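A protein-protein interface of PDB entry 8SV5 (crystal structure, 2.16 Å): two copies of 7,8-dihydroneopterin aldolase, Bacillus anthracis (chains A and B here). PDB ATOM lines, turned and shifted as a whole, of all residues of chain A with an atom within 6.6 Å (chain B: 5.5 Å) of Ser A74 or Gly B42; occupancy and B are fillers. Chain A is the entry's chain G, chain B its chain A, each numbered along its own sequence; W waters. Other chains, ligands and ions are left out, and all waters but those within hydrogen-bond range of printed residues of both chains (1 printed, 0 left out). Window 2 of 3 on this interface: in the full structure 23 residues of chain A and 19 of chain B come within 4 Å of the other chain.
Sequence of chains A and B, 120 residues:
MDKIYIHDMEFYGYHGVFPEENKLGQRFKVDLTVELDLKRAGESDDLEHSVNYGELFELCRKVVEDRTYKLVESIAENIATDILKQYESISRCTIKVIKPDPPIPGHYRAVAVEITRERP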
ATOM      1  N   VAL A  63     -20.789 -13.791 -21.797  1.00  0.00           N
ATOM      2  CA  VAL A  63     -19.676 -14.668 -22.146  1.00  0.00           C
ATOM      3  C   VAL A  63     -18.431 -13.851 -22.465  1.00  0.00           C
ATOM      4  O   VAL A  63     -17.316 -14.209 -22.067  1.00  0.00           O
ATOM      5  CB  VAL A  63     -20.065 -15.604 -23.308  1.00  0.00           C
ATOM      6  CG1 VAL A  63     -18.928 -16.571 -23.611  1.00  0.00           C
ATOM      7  CG2 VAL A  63     -21.345 -16.368 -22.981  1.00  0.00           C
ATOM      8  N   TYR A  69     -11.383 -16.311 -20.931  1.00  0.00           N
ATOM      9  CA  TYR A  69     -10.898 -17.550 -21.506  1.00  0.00           C
ATOM     10  C   TYR A  69      -9.588 -17.257 -22.223  1.00  0.00           C
ATOM     11  O   TYR A  69      -9.267 -16.104 -22.525  1.00  0.00           O
ATOM     12  CB  TYR A  69     -11.891 -18.123 -22.527  1.00  0.00           C
ATOM     13  CG  TYR A  69     -13.257 -18.441 -21.968  1.00  0.00           C
ATOM     14  CD1 TYR A  69     -13.456 -19.553 -21.160  1.00  0.00           C
ATOM     15  CD2 TYR A  69     -14.351 -17.638 -22.257  1.00  0.00           C
ATOM     16  CE1 TYR A  69     -14.705 -19.852 -20.650  1.00  0.00           C
ATOM     17  CE2 TYR A  69     -15.605 -17.928 -21.751  1.00  0.00           C
ATOM     18  CZ  TYR A  69     -15.776 -19.037 -20.949  1.00  0.00           C
ATOM     19  OH  TYR A  69     -17.020 -19.330 -20.444  1.00  0.00           O
ATOM     20  N   LYS A  70      -8.831 -18.314 -22.498  1.00  0.00           N
ATOM     21  CA  LYS A  70      -7.607 -18.142 -23.269  1.00  0.00           C
ATOM     22  C   LYS A  70      -7.899 -18.086 -24.764  1.00  0.00           C
ATOM     23  O   LYS A  70      -7.262 -17.317 -25.495  1.00  0.00           O
ATOM     24  CB  LYS A  70      -6.630 -19.270 -22.950  1.00  0.00           C
ATOM     25  CG  LYS A  70      -5.976 -19.139 -21.583  1.00  0.00           C
ATOM     26  CD  LYS A  70      -5.817 -20.489 -20.903  1.00  0.00           C
ATOM     27  CE  LYS A  70      -4.833 -21.381 -21.646  1.00  0.00           C
ATOM     28  NZ  LYS A  70      -5.340 -22.775 -21.771  1.00  0.00           N
ATOM     29  N   LEU A  71      -8.868 -18.869 -25.230  1.00  0.00           N
ATOM     30  CA  LEU A  71      -9.159 -19.006 -26.647  1.00  0.00           C
ATOM     31  C   LEU A  71     -10.495 -18.365 -26.993  1.00  0.00           C
ATOM     32  O   LEU A  71     -11.477 -18.510 -26.257  1.00  0.00           O
ATOM     33  CB  LEU A  71      -9.219 -20.485 -27.038  1.00  0.00           C
ATOM     34  CG  LEU A  71      -8.030 -21.349 -26.629  1.00  0.00           C
ATOM     35  CD1 LEU A  71      -8.170 -22.739 -27.231  1.00  0.00           C
ATOM     36  CD2 LEU A  71      -6.719 -20.706 -27.053  1.00  0.00           C
ATOM     37  N   VAL A  72     -10.526 -17.657 -28.127  1.00  0.00           N
ATOM     38  CA  VAL A  72     -11.799 -17.225 -28.693  1.00  0.00           C
ATOM     39  C   VAL A  72     -12.662 -18.435 -29.030  1.00  0.00           C
ATOM     40  O   VAL A  72     -13.895 -18.338 -29.075  1.00  0.00           O
ATOM     41  CB  VAL A  72     -11.577 -16.318 -29.921  1.00  0.00           C
ATOM     42  CG1 VAL A  72     -11.096 -14.941 -29.482  1.00  0.00           C
ATOM     43  CG2 VAL A  72     -10.593 -16.948 -30.903  1.00  0.00           C
ATOM     44  N   GLU A  73     -12.033 -19.588 -29.277  1.00  0.00           N
ATOM     45  CA  GLU A  73     -12.786 -20.826 -29.441  1.00  0.00           C
ATOM     46  C   GLU A  73     -13.724 -21.055 -28.263  1.00  0.00           C
ATOM     47  O   GLU A  73     -14.867 -21.492 -28.442  1.00  0.00           O
ATOM     48  CB  GLU A  73     -11.817 -22.003 -29.568  1.00  0.00           C
ATOM     49  CG  GLU A  73     -11.282 -22.230 -30.973  1.00  0.00           C
ATOM     50  CD  GLU A  73      -9.948 -21.546 -31.213  1.00  0.00           C
ATOM     51  OE1 GLU A  73      -9.646 -20.553 -30.517  1.00  0.00           O
ATOM     52  OE2 GLU A  73      -9.201 -22.004 -32.103  1.00  0.00           O
ATOM     53  N   SER A  74     -13.255 -20.770 -27.045  1.00  0.00           N
ATOM     54  CA  SER A  74     -14.086 -20.984 -25.864  1.00  0.00           C
ATOM     55  C   SER A  74     -15.245 -19.997 -25.818  1.00  0.00           C
ATOM     56  O   SER A  74     -16.359 -20.360 -25.422  1.00  0.00           O
ATOM     57  CB  SER A  74     -13.233 -20.873 -24.600  1.00  0.00           C
ATOM     58  OG  SER A  74     -12.245 -21.888 -24.573  1.00  0.00           O
ATOM     59  N   ILE A  75     -15.002 -18.746 -26.213  1.00  0.00           N
ATOM     60  CA  ILE A  75     -16.082 -17.764 -26.291  1.00  0.00           C
ATOM     61  C   ILE A  75     -17.178 -18.271 -27.217  1.00  0.00           C
ATOM     62  O   ILE A  75     -18.354 -18.355 -26.839  1.00  0.00           O
ATOM     63  CB  ILE A  75     -15.538 -16.405 -26.764  1.00  0.00           C
ATOM     64  CG1 ILE A  75     -14.522 -15.853 -25.764  1.00  0.00           C
ATOM     65  CG2 ILE A  75     -16.674 -15.405 -26.962  1.00  0.00           C
ATOM     66  CD1 ILE A  75     -13.658 -14.759 -26.339  1.00  0.00           C
ATOM     67  N   ALA A  76     -16.805 -18.617 -28.449  1.00  0.00           N
ATOM     68  CA  ALA A  76     -17.789 -19.079 -29.420  1.00  0.00           C
ATOM     69  C   ALA A  76     -18.541 -20.297 -28.901  1.00  0.00           C
ATOM     70  O   ALA A  76     -19.770 -20.368 -28.991  1.00  0.00           O
ATOM     71  CB  ALA A  76     -17.106 -19.390 -30.750  1.00  0.00           C
ATOM     72  N   GLU A  77     -17.814 -21.269 -28.340  1.00  0.00           N
ATOM     73  CA  GLU A  77     -18.459 -22.499 -27.894  1.00  0.00           C
ATOM     74  C   GLU A  77     -19.416 -22.248 -26.736  1.00  0.00           C
ATOM     75  O   GLU A  77     -20.455 -22.911 -26.639  1.00  0.00           O
ATOM     76  CB  GLU A  77     -17.404 -23.534 -27.499  1.00  0.00           C
ATOM     77  CG  GLU A  77     -17.957 -24.933 -27.261  1.00  0.00           C
ATOM     78  CD  GLU A  77     -18.453 -25.596 -28.535  1.00  0.00           C
ATOM     79  OE1 GLU A  77     -17.691 -25.640 -29.525  1.00  0.00           O
ATOM     80  OE2 GLU A  77     -19.605 -26.077 -28.547  1.00  0.00           O
ATOM     81  N   ASN A  78     -19.095 -21.300 -25.855  1.00  0.00           N
ATOM     82  CA  ASN A  78     -19.949 -21.050 -24.699  1.00  0.00           C
ATOM     83  C   ASN A  78     -21.195 -20.256 -25.069  1.00  0.00           C
ATOM     84  O   ASN A  78     -22.254 -20.460 -24.463  1.00  0.00           O
ATOM     85  CB  ASN A  78     -19.156 -20.337 -23.603  1.00  0.00           C
ATOM     86  CG  ASN A  78     -18.471 -21.308 -22.656  1.00  0.00           C
ATOM     87  OD1 ASN A  78     -19.128 -22.088 -21.967  1.00  0.00           O
ATOM     88  ND2 ASN A  78     -17.145 -21.260 -22.617  1.00  0.00           N
ATOM     89  N   ILE A  79     -21.098 -19.356 -26.050  1.00  0.00           N
ATOM     90  CA  ILE A  79     -22.291 -18.662 -26.534  1.00  0.00           C
ATOM     91  C   ILE A  79     -23.244 -19.655 -27.188  1.00  0.00           C
ATOM     92  O   ILE A  79     -24.440 -19.694 -26.878  1.00  0.00           O
ATOM     93  CB  ILE A  79     -21.901 -17.524 -27.498  1.00  0.00           C
ATOM     94  CG1 ILE A  79     -21.141 -16.430 -26.743  1.00  0.00           C
ATOM     95  CG2 ILE A  79     -23.143 -16.944 -28.184  1.00  0.00           C
ATOM     96  CD1 ILE A  79     -20.624 -15.305 -27.630  1.00  0.00           C
ATOM     97  N   VAL A 113     -12.806 -16.771 -35.310  1.00  0.00           N
ATOM     98  CA  VAL A 113     -13.229 -18.164 -35.315  1.00  0.00           C
ATOM     99  C   VAL A 113     -14.740 -18.184 -35.500  1.00  0.00           C
ATOM    100  O   VAL A 113     -15.451 -17.325 -34.967  1.00  0.00           O
ATOM    101  CB  VAL A 113     -12.827 -18.896 -34.017  1.00  0.00           C
ATOM    102  CG1 VAL A 113     -11.335 -18.777 -33.782  1.00  0.00           C
ATOM    103  CG2 VAL A 113     -13.596 -18.348 -32.821  1.00  0.00           C
ATOM    104  N   LEU B  38     -13.205 -27.348 -33.986  1.00  0.00           N
ATOM    105  CA  LEU B  38     -12.812 -26.481 -32.889  1.00  0.00           C
ATOM    106  C   LEU B  38     -13.548 -26.800 -31.596  1.00  0.00           C
ATOM    107  O   LEU B  38     -13.286 -26.154 -30.576  1.00  0.00           O
ATOM    108  CB  LEU B  38     -13.044 -25.016 -33.271  1.00  0.00           C
ATOM    109  CG  LEU B  38     -12.144 -24.490 -34.391  1.00  0.00           C
ATOM    110  CD1 LEU B  38     -12.490 -23.046 -34.714  1.00  0.00           C
ATOM    111  CD2 LEU B  38     -10.671 -24.612 -34.023  1.00  0.00           C
ATOM    112  N   LYS B  39     -14.449 -27.784 -31.607  1.00  0.00           N
ATOM    113  CA  LYS B  39     -15.223 -28.098 -30.411  1.00  0.00           C
ATOM    114  C   LYS B  39     -14.304 -28.395 -29.230  1.00  0.00           C
ATOM    115  O   LYS B  39     -14.336 -27.693 -28.213  1.00  0.00           O
ATOM    116  CB  LYS B  39     -16.170 -29.269 -30.685  1.00  0.00           C
ATOM    117  CG  LYS B  39     -17.387 -29.292 -29.771  1.00  0.00           C
ATOM    118  CD  LYS B  39     -18.410 -30.326 -30.217  1.00  0.00           C
ATOM    119  CE  LYS B  39     -19.697 -30.217 -29.413  1.00  0.00           C
ATOM    120  NZ  LYS B  39     -20.904 -30.186 -30.283  1.00  0.00           N
ATOM    121  N   ARG B  40     -13.457 -29.421 -29.354  1.00  0.00           N
ATOM    122  CA  ARG B  40     -12.592 -29.792 -28.237  1.00  0.00           C
ATOM    123  C   ARG B  40     -11.783 -28.598 -27.744  1.00  0.00           C
ATOM    124  O   ARG B  40     -11.551 -28.450 -26.538  1.00  0.00           O
ATOM    125  CB  ARG B  40     -11.664 -30.946 -28.624  1.00  0.00           C
ATOM    126  CG  ARG B  40     -10.975 -31.588 -27.421  1.00  0.00           C
ATOM    127  CD  ARG B  40     -10.014 -32.699 -27.822  1.00  0.00           C
ATOM    128  NE  ARG B  40     -10.704 -33.885 -28.314  1.00  0.00           N
ATOM    129  CZ  ARG B  40     -11.435 -34.700 -27.563  1.00  0.00           C
ATOM    130  NH1 ARG B  40     -11.603 -34.482 -26.269  1.00  0.00           N
ATOM    131  NH2 ARG B  40     -12.011 -35.758 -28.125  1.00  0.00           N
ATOM    132  N   ALA B  41     -11.355 -27.728 -28.661  1.00  0.00           N
ATOM    133  CA  ALA B  41     -10.611 -26.536 -28.261  1.00  0.00           C
ATOM    134  C   ALA B  41     -11.481 -25.608 -27.423  1.00  0.00           C
ATOM    135  O   ALA B  41     -11.053 -25.114 -26.373  1.00  0.00           O
ATOM    136  CB  ALA B  41     -10.081 -25.809 -29.496  1.00  0.00           C
ATOM    137  N   GLY B  42     -12.709 -25.352 -27.875  1.00  0.00           N
ATOM    138  CA  GLY B  42     -13.633 -24.565 -27.081  1.00  0.00           C
ATOM    139  C   GLY B  42     -14.103 -25.268 -25.826  1.00  0.00           C
ATOM    140  O   GLY B  42     -14.487 -24.600 -24.860  1.00  0.00           O
ATOM    141  N   GLU B  43     -14.082 -26.602 -25.820  1.00  0.00           N
ATOM    142  CA  GLU B  43     -14.438 -27.344 -24.618  1.00  0.00           C
ATOM    143  C   GLU B  43     -13.324 -27.264 -23.577  1.00  0.00           C
ATOM    144  O   GLU B  43     -13.595 -27.154 -22.376  1.00  0.00           O
ATOM    145  CB  GLU B  43     -14.711 -28.808 -24.970  1.00  0.00           C
ATOM    146  CG  GLU B  43     -15.903 -29.067 -25.894  1.00  0.00           C
ATOM    147  CD  GLU B  43     -17.242 -28.682 -25.292  1.00  0.00           C
ATOM    148  OE1 GLU B  43     -17.271 -27.880 -24.338  1.00  0.00           O
ATOM    149  OE2 GLU B  43     -18.273 -29.186 -25.784  1.00  0.00           O
ATOM    150  N   SER B  44     -12.068 -27.307 -24.022  1.00  0.00           N
ATOM    151  CA  SER B  44     -10.930 -27.397 -23.121  1.00  0.00           C
ATOM    152  C   SER B  44     -10.193 -26.078 -22.927  1.00  0.00           C
ATOM    153  O   SER B  44      -9.459 -25.941 -21.943  1.00  0.00           O
ATOM    154  CB  SER B  44      -9.932 -28.431 -23.655  1.00  0.00           C
ATOM    155  OG  SER B  44      -9.390 -28.004 -24.893  1.00  0.00           O
ATOM    156  N   ASP B  45     -10.364 -25.113 -23.831  1.00  0.00           N
ATOM    157  CA  ASP B  45      -9.632 -23.848 -23.769  1.00  0.00           C
ATOM    158  C   ASP B  45      -8.127 -24.067 -23.908  1.00  0.00           C
ATOM    159  O   ASP B  45      -7.324 -23.332 -23.327  1.00  0.00           O
ATOM    160  CB  ASP B  45      -9.947 -23.076 -22.481  1.00  0.00           C
ATOM    161  CG  ASP B  45      -9.764 -21.575 -22.638  1.00  0.00           C
ATOM    162  OD1 ASP B  45      -9.710 -21.092 -23.791  1.00  0.00           O
ATOM    163  OD2 ASP B  45      -9.683 -20.875 -21.607  1.00  0.00           O
HETATM  164  O   HOH W   1     -14.866 -23.706 -21.856  1.00  0.00           O
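No position is printed for both chains.
Of the 11 pairs that touch across the chains among the printed residues, none has its exchanged pair printed and touching as well.
Of chain B, only Ala B41, Gly B42 and Asp B45 come within 4 Å of Ser A74.
Gly B42 touches just these residues of chain A: Glu A73 (3.6 Å), Ser A74 (3.5 Å) and Glu A77 (3.9 Å).
Of the printed residues of chain A, Leu B38 touches Glu A73.
Of the printed residues of chain B, Leu A71 touches Ala B41 and Asp B45.
Printed residues of chain B within 4 Å of Lys A70: Asp B45 (2.6 Å).
Printed residues of chain A within 4 Å of Lys B39: Glu A77 (3.6 Å).
Of the printed residues of chain A, Ala B41 touches Leu A71 (3.8 Å) and Ser A74 (3.9 Å).
The nearest residue of chain B that does not touch Ser A74 is Ser B44 (4.9 Å).
The nearest printed residue of chain B that does not touch Tyr A69 is Gly B42 (6.3 Å).
O of Ser A74 is in hydrogen-bond range of ND2 of Asn A78 (3.0 Å).
OH of Tyr A69 lies within hydrogen-bond range of ND2 of Asn A78 (2.9 Å).
N of Leu A71 lies within hydrogen-bond range of OD1 of Asp B45 (2.8 Å).
The side-chain carboxylate (OD1) of Asp B45 sits at hydrogen-bond distance from the side-chain hydroxyl (OG) of Ser A74, at 2.8 Å.
NZ of Lys A70 lies within hydrogen-bond range of O of Asp B45, at 2.6 Å.
Water W1 lies within hydrogen-bond range of O of Gly B42 (3.2 Å) and ND2 of Asn A78 (3.4 Å).
Tyr A69 touches Asp B45.
CD1 of Leu A71 touches O of Ala B41 (3.8 Å).
Leu B38 touches Glu A73.
Gly B42 touches Glu A73.
Ser A74 touches Ala B41.
Ser A74 touches Gly B42 (OG to O, 3.5 Å).
Glu A77 touches Lys B39 (OE1 to CA, 3.6 Å).
Glu A77 touches Gly B42 (CB to CA, 3.9 Å).
Printed residues of chain A that touch a printed residue of chain B: Tyr A69, Lys A70, Leu A71, Glu A73, Ser A74 and Glu A77.
Hydrophobic or aromatic side chains of chain A within 4 Å of the printed part of chain B: Tyr A69 and Leu A71.
Of the 8 printed residues of chain B, 5 touch a printed residue of chain A.
Hydrophobic or aromatic side chains of chain B that line the printed part of chain A: Leu B38.
Among the printed residues, no Asp or Glu carboxylate lies within 4 Å of a Lys or Arg side-chain nitrogen of the other chain.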
